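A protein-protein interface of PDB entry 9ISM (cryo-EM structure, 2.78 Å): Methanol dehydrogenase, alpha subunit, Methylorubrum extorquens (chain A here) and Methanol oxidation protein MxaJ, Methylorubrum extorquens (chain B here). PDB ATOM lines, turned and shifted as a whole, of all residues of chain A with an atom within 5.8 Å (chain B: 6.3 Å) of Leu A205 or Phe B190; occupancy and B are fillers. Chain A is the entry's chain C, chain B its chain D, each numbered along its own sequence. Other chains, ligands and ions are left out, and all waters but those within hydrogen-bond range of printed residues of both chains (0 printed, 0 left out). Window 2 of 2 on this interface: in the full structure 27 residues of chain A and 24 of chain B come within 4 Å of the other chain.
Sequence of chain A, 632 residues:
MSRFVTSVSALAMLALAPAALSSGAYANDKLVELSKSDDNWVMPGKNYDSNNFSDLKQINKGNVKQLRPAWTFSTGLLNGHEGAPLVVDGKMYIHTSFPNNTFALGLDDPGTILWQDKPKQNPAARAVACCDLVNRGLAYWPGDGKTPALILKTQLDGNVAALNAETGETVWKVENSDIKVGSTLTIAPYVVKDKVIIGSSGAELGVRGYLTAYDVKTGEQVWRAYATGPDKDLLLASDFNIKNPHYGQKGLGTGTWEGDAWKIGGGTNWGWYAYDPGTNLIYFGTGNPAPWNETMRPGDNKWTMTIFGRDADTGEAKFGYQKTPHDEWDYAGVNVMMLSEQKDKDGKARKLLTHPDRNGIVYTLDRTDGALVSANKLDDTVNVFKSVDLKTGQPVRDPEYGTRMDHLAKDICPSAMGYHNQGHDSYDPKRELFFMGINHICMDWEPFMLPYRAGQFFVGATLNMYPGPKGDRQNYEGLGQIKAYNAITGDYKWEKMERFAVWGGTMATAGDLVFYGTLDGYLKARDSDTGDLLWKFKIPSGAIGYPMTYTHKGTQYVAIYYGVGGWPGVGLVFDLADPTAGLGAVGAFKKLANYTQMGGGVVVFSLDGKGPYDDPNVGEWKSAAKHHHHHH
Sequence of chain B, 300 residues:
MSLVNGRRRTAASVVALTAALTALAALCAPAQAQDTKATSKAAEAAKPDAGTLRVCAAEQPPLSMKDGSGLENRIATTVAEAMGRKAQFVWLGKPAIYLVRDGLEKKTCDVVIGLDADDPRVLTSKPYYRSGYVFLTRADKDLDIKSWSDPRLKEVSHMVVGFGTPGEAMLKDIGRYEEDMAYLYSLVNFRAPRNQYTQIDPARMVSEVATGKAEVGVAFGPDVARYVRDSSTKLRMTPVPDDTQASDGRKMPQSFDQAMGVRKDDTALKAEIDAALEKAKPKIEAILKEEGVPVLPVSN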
ATOM      1  N   ALA A 127     -24.489 -21.625  -7.483  1.00  0.00           N
ATOM      2  CA  ALA A 127     -24.347 -20.221  -7.113  1.00  0.00           C
ATOM      3  C   ALA A 127     -23.265 -19.532  -7.937  1.00  0.00           C
ATOM      4  O   ALA A 127     -23.438 -18.384  -8.364  1.00  0.00           O
ATOM      5  CB  ALA A 127     -24.044 -20.102  -5.622  1.00  0.00           C
ATOM      6  N   VAL A 128     -22.142 -20.212  -8.165  1.00  0.00           N
ATOM      7  CA  VAL A 128     -21.013 -19.586  -8.845  1.00  0.00           C
ATOM      8  C   VAL A 128     -21.338 -19.328 -10.312  1.00  0.00           C
ATOM      9  O   VAL A 128     -21.108 -18.231 -10.831  1.00  0.00           O
ATOM     10  CB  VAL A 128     -19.751 -20.452  -8.692  1.00  0.00           C
ATOM     11  CG1 VAL A 128     -18.696 -20.042  -9.704  1.00  0.00           C
ATOM     12  CG2 VAL A 128     -19.210 -20.350  -7.277  1.00  0.00           C
ATOM     13  N   ILE A 179     -13.960 -24.872  -7.225  1.00  0.00           N
ATOM     14  CA  ILE A 179     -15.108 -23.972  -7.209  1.00  0.00           C
ATOM     15  C   ILE A 179     -14.764 -22.663  -6.507  1.00  0.00           C
ATOM     16  O   ILE A 179     -15.239 -21.594  -6.909  1.00  0.00           O
ATOM     17  CB  ILE A 179     -16.316 -24.670  -6.558  1.00  0.00           C
ATOM     18  CG1 ILE A 179     -16.818 -25.798  -7.457  1.00  0.00           C
ATOM     19  CG2 ILE A 179     -17.439 -23.683  -6.291  1.00  0.00           C
ATOM     20  CD1 ILE A 179     -17.312 -25.323  -8.803  1.00  0.00           C
ATOM     21  N   LYS A 180     -13.932 -22.720  -5.465  1.00  0.00           N
ATOM     22  CA  LYS A 180     -13.611 -21.519  -4.699  1.00  0.00           C
ATOM     23  C   LYS A 180     -12.938 -20.465  -5.571  1.00  0.00           C
ATOM     24  O   LYS A 180     -13.234 -19.270  -5.450  1.00  0.00           O
ATOM     25  CB  LYS A 180     -12.724 -21.880  -3.510  1.00  0.00           C
ATOM     26  CG  LYS A 180     -13.397 -22.788  -2.496  1.00  0.00           C
ATOM     27  CD  LYS A 180     -12.409 -23.280  -1.452  1.00  0.00           C
ATOM     28  CE  LYS A 180     -11.455 -24.308  -2.038  1.00  0.00           C
ATOM     29  NZ  LYS A 180     -12.180 -25.371  -2.787  1.00  0.00           N
ATOM     30  N   VAL A 181     -12.026 -20.885  -6.447  1.00  0.00           N
ATOM     31  CA  VAL A 181     -11.429 -19.951  -7.397  1.00  0.00           C
ATOM     32  C   VAL A 181     -12.488 -19.423  -8.356  1.00  0.00           C
ATOM     33  O   VAL A 181     -12.521 -18.228  -8.672  1.00  0.00           O
ATOM     34  CB  VAL A 181     -10.264 -20.624  -8.146  1.00  0.00           C
ATOM     35  CG1 VAL A 181      -9.970 -19.899  -9.448  1.00  0.00           C
ATOM     36  CG2 VAL A 181      -9.024 -20.668  -7.264  1.00  0.00           C
ATOM     37  N   GLY A 182     -13.371 -20.298  -8.826  1.00  0.00           N
ATOM     38  CA  GLY A 182     -14.464 -19.883  -9.682  1.00  0.00           C
ATOM     39  C   GLY A 182     -14.526 -20.627 -10.999  1.00  0.00           C
ATOM     40  O   GLY A 182     -15.177 -20.173 -11.943  1.00  0.00           O
ATOM     41  N   ALA A 203     -15.185 -18.849 -14.752  1.00  0.00           N
ATOM     42  CA  ALA A 203     -15.478 -17.423 -14.752  1.00  0.00           C
ATOM     43  C   ALA A 203     -14.329 -16.573 -15.272  1.00  0.00           C
ATOM     44  O   ALA A 203     -14.523 -15.369 -15.469  1.00  0.00           O
ATOM     45  CB  ALA A 203     -15.854 -16.965 -13.341  1.00  0.00           C
ATOM     46  N   GLU A 204     -13.147 -17.163 -15.477  1.00  0.00           N
ATOM     47  CA  GLU A 204     -11.971 -16.490 -16.049  1.00  0.00           C
ATOM     48  C   GLU A 204     -11.715 -15.120 -15.416  1.00  0.00           C
ATOM     49  O   GLU A 204     -11.221 -14.196 -16.068  1.00  0.00           O
ATOM     50  CB  GLU A 204     -12.079 -16.387 -17.579  1.00  0.00           C
ATOM     51  CG  GLU A 204     -13.084 -15.382 -18.130  1.00  0.00           C
ATOM     52  CD  GLU A 204     -13.368 -15.589 -19.604  1.00  0.00           C
ATOM     53  OE1 GLU A 204     -12.479 -16.103 -20.316  1.00  0.00           O
ATOM     54  OE2 GLU A 204     -14.481 -15.240 -20.053  1.00  0.00           O
ATOM     55  N   LEU A 205     -12.019 -14.989 -14.125  1.00  0.00           N
ATOM     56  CA  LEU A 205     -11.800 -13.723 -13.433  1.00  0.00           C
ATOM     57  C   LEU A 205     -10.361 -13.601 -12.943  1.00  0.00           C
ATOM     58  O   LEU A 205      -9.642 -12.671 -13.320  1.00  0.00           O
ATOM     59  CB  LEU A 205     -12.785 -13.583 -12.271  1.00  0.00           C
ATOM     60  CG  LEU A 205     -14.176 -13.082 -12.667  1.00  0.00           C
ATOM     61  CD1 LEU A 205     -15.115 -13.066 -11.474  1.00  0.00           C
ATOM     62  CD2 LEU A 205     -14.092 -11.705 -13.303  1.00  0.00           C
ATOM     63  N   GLY A 206      -9.924 -14.534 -12.102  1.00  0.00           N
ATOM     64  CA  GLY A 206      -8.592 -14.461 -11.533  1.00  0.00           C
ATOM     65  C   GLY A 206      -7.776 -15.733 -11.650  1.00  0.00           C
ATOM     66  O   GLY A 206      -7.025 -16.073 -10.733  1.00  0.00           O
ATOM     67  N   VAL A 207      -7.908 -16.447 -12.768  1.00  0.00           N
ATOM     68  CA  VAL A 207      -7.174 -17.689 -12.977  1.00  0.00           C
ATOM     69  C   VAL A 207      -6.846 -17.819 -14.456  1.00  0.00           C
ATOM     70  O   VAL A 207      -7.537 -17.265 -15.314  1.00  0.00           O
ATOM     71  CB  VAL A 207      -7.976 -18.909 -12.463  1.00  0.00           C
ATOM     72  CG1 VAL A 207      -9.099 -19.264 -13.427  1.00  0.00           C
ATOM     73  CG2 VAL A 207      -7.057 -20.102 -12.225  1.00  0.00           C
ATOM     74  N   ILE A 264      -3.028 -13.721 -14.256  1.00  0.00           N
ATOM     75  CA  ILE A 264      -4.457 -13.479 -14.396  1.00  0.00           C
ATOM     76  C   ILE A 264      -4.832 -13.341 -15.875  1.00  0.00           C
ATOM     77  O   ILE A 264      -5.885 -12.822 -16.217  1.00  0.00           O
ATOM     78  CB  ILE A 264      -4.882 -12.248 -13.570  1.00  0.00           C
ATOM     79  CG1 ILE A 264      -4.433 -12.411 -12.125  1.00  0.00           C
ATOM     80  CG2 ILE A 264      -6.394 -12.120 -13.485  1.00  0.00           C
ATOM     81  CD1 ILE A 264      -4.577 -11.155 -11.309  1.00  0.00           C
ATOM     82  N   ALA A 290      -7.816 -11.737 -20.209  1.00  0.00           N
ATOM     83  CA  ALA A 290      -8.519 -11.038 -19.148  1.00  0.00           C
ATOM     84  C   ALA A 290      -7.561 -10.099 -18.434  1.00  0.00           C
ATOM     85  O   ALA A 290      -6.350 -10.341 -18.419  1.00  0.00           O
ATOM     86  CB  ALA A 290      -9.121 -12.028 -18.141  1.00  0.00           C
ATOM     87  N   MET B 181      -7.087 -11.196  -5.993  1.00  0.00           N
ATOM     88  CA  MET B 181      -8.177 -10.857  -6.903  1.00  0.00           C
ATOM     89  C   MET B 181      -9.293 -11.893  -6.844  1.00  0.00           C
ATOM     90  O   MET B 181     -10.481 -11.541  -6.843  1.00  0.00           O
ATOM     91  CB  MET B 181      -7.641 -10.711  -8.324  1.00  0.00           C
ATOM     92  CG  MET B 181      -8.676 -10.277  -9.344  1.00  0.00           C
ATOM     93  SD  MET B 181      -7.931 -10.038 -10.965  1.00  0.00           S
ATOM     94  CE  MET B 181      -9.362  -9.644 -11.961  1.00  0.00           C
ATOM     95  N   ALA B 182      -8.931 -13.177  -6.792  1.00  0.00           N
ATOM     96  CA  ALA B 182      -9.939 -14.228  -6.695  1.00  0.00           C
ATOM     97  C   ALA B 182     -10.723 -14.127  -5.394  1.00  0.00           C
ATOM     98  O   ALA B 182     -11.943 -14.316  -5.382  1.00  0.00           O
ATOM     99  CB  ALA B 182      -9.278 -15.600  -6.820  1.00  0.00           C
ATOM    100  N   TYR B 185     -13.182 -11.210  -5.732  1.00  0.00           N
ATOM    101  CA  TYR B 185     -14.318 -11.581  -6.570  1.00  0.00           C
ATOM    102  C   TYR B 185     -15.127 -12.738  -6.002  1.00  0.00           C
ATOM    103  O   TYR B 185     -16.200 -13.030  -6.533  1.00  0.00           O
ATOM    104  CB  TYR B 185     -13.863 -11.912  -7.991  1.00  0.00           C
ATOM    105  CG  TYR B 185     -13.583 -10.695  -8.839  1.00  0.00           C
ATOM    106  CD1 TYR B 185     -14.060  -9.447  -8.469  1.00  0.00           C
ATOM    107  CD2 TYR B 185     -12.856 -10.794 -10.013  1.00  0.00           C
ATOM    108  CE1 TYR B 185     -13.814  -8.331  -9.242  1.00  0.00           C
ATOM    109  CE2 TYR B 185     -12.606  -9.682 -10.791  1.00  0.00           C
ATOM    110  CZ  TYR B 185     -13.087  -8.453 -10.400  1.00  0.00           C
ATOM    111  OH  TYR B 185     -12.838  -7.343 -11.172  1.00  0.00           O
ATOM    112  N   SER B 186     -14.638 -13.410  -4.961  1.00  0.00           N
ATOM    113  CA  SER B 186     -15.418 -14.448  -4.304  1.00  0.00           C
ATOM    114  C   SER B 186     -16.211 -13.936  -3.114  1.00  0.00           C
ATOM    115  O   SER B 186     -17.162 -14.603  -2.693  1.00  0.00           O
ATOM    116  CB  SER B 186     -14.509 -15.589  -3.840  1.00  0.00           C
ATOM    117  OG  SER B 186     -13.625 -15.155  -2.823  1.00  0.00           O
ATOM    118  N   LEU B 187     -15.839 -12.781  -2.554  1.00  0.00           N
ATOM    119  CA  LEU B 187     -16.629 -12.215  -1.462  1.00  0.00           C
ATOM    120  C   LEU B 187     -18.062 -11.953  -1.901  1.00  0.00           C
ATOM    121  O   LEU B 187     -19.009 -12.228  -1.157  1.00  0.00           O
ATOM    122  CB  LEU B 187     -15.981 -10.935  -0.947  1.00  0.00           C
ATOM    123  CG  LEU B 187     -14.627 -11.147  -0.280  1.00  0.00           C
ATOM    124  CD1 LEU B 187     -13.999  -9.819   0.069  1.00  0.00           C
ATOM    125  CD2 LEU B 187     -14.788 -12.005   0.958  1.00  0.00           C
ATOM    126  N   VAL B 188     -18.240 -11.419  -3.100  1.00  0.00           N
ATOM    127  CA  VAL B 188     -19.524 -11.436  -3.770  1.00  0.00           C
ATOM    128  C   VAL B 188     -19.483 -12.607  -4.743  1.00  0.00           C
ATOM    129  O   VAL B 188     -18.420 -13.147  -5.053  1.00  0.00           O
ATOM    130  CB  VAL B 188     -19.824 -10.098  -4.491  1.00  0.00           C
ATOM    131  CG1 VAL B 188     -18.842  -9.862  -5.627  1.00  0.00           C
ATOM    132  CG2 VAL B 188     -21.270 -10.024  -4.971  1.00  0.00           C
ATOM    133  N   ASN B 189     -20.651 -13.034  -5.212  1.00  0.00           N
ATOM    134  CA  ASN B 189     -20.678 -14.074  -6.228  1.00  0.00           C
ATOM    135  C   ASN B 189     -19.998 -13.568  -7.493  1.00  0.00           C
ATOM    136  O   ASN B 189     -19.955 -12.365  -7.762  1.00  0.00           O
ATOM    137  CB  ASN B 189     -22.115 -14.497  -6.525  1.00  0.00           C
ATOM    138  CG  ASN B 189     -22.897 -14.817  -5.268  1.00  0.00           C
ATOM    139  OD1 ASN B 189     -24.065 -14.452  -5.140  1.00  0.00           O
ATOM    140  ND2 ASN B 189     -22.253 -15.497  -4.328  1.00  0.00           N
ATOM    141  N   PHE B 190     -19.458 -14.497  -8.278  1.00  0.00           N
ATOM    142  CA  PHE B 190     -18.636 -14.112  -9.417  1.00  0.00           C
ATOM    143  C   PHE B 190     -19.503 -13.527 -10.521  1.00  0.00           C
ATOM    144  O   PHE B 190     -19.624 -14.106 -11.604  1.00  0.00           O
ATOM    145  CB  PHE B 190     -17.842 -15.311  -9.936  1.00  0.00           C
ATOM    146  CG  PHE B 190     -16.874 -15.873  -8.938  1.00  0.00           C
ATOM    147  CD1 PHE B 190     -17.301 -16.745  -7.953  1.00  0.00           C
ATOM    148  CD2 PHE B 190     -15.536 -15.535  -8.987  1.00  0.00           C
ATOM    149  CE1 PHE B 190     -16.413 -17.262  -7.037  1.00  0.00           C
ATOM    150  CE2 PHE B 190     -14.646 -16.050  -8.073  1.00  0.00           C
ATOM    151  CZ  PHE B 190     -15.085 -16.915  -7.098  1.00  0.00           C
ATOM    152  N   ARG B 191     -20.100 -12.366 -10.252  1.00  0.00           N
ATOM    153  CA  ARG B 191     -21.023 -11.702 -11.172  1.00  0.00           C
ATOM    154  C   ARG B 191     -20.707 -10.209 -11.135  1.00  0.00           C
ATOM    155  O   ARG B 191     -21.220  -9.477 -10.285  1.00  0.00           O
ATOM    156  CB  ARG B 191     -22.471 -11.983 -10.794  1.00  0.00           C
ATOM    157  CG  ARG B 191     -23.430 -12.009 -11.968  1.00  0.00           C
ATOM    158  CD  ARG B 191     -24.798 -12.529 -11.550  1.00  0.00           C
ATOM    159  NE  ARG B 191     -25.734 -12.593 -12.668  1.00  0.00           N
ATOM    160  CZ  ARG B 191     -25.652 -13.454 -13.673  1.00  0.00           C
ATOM    161  NH1 ARG B 191     -24.694 -14.366 -13.727  1.00  0.00           N
ATOM    162  NH2 ARG B 191     -26.558 -13.405 -14.645  1.00  0.00           N
ATOM    163  N   ALA B 192     -19.859  -9.766 -12.059  1.00  0.00           N
ATOM    164  CA  ALA B 192     -19.470  -8.362 -12.175  1.00  0.00           C
ATOM    165  C   ALA B 192     -19.618  -7.917 -13.623  1.00  0.00           C
ATOM    166  O   ALA B 192     -18.626  -7.754 -14.343  1.00  0.00           O
ATOM    167  CB  ALA B 192     -18.041  -8.146 -11.678  1.00  0.00           C
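O of Gly A182 lies within hydrogen-bond range of N of Ala A203, at 3.1 Å.
Among the printed residues, pairs that only touch across the chains: Val A181 with Phe B190, Leu A205 with Met B181, Lys A180 with Phe B190, Leu A205 with Tyr B185, Leu A205 with Phe B190, Ile A264 with Met B181, Gly A182 with Phe B190 and Val A128 with Phe B190.
Of the printed residues of chain A, Phe B190 touches Val A128, Lys A180, Val A181, Gly A182 and Leu A205. Of the printed residues of chain A, Met B181 touches Leu A205 (3.3 Å) and Ile A264 (3.6 Å). Of the printed residues of chain B, Lys A180 touches Phe B190 (3.4 Å). Ala A290 touches none of the printed residues of chain B. Leu B187 touches none of the printed residues of chain A. The nearest residue of chain B that does not touch Leu A205 is Arg B191 (5.2 Å).
Hydrophobic or aromatic side chains of chain B within 4 Å of the printed part of chain A: Met B181, Tyr B185 and Phe B190. Among the printed residues, no Asp or Glu carboxylate lies within 4 Å of a Lys or Arg side-chain nitrogen of the other chain.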
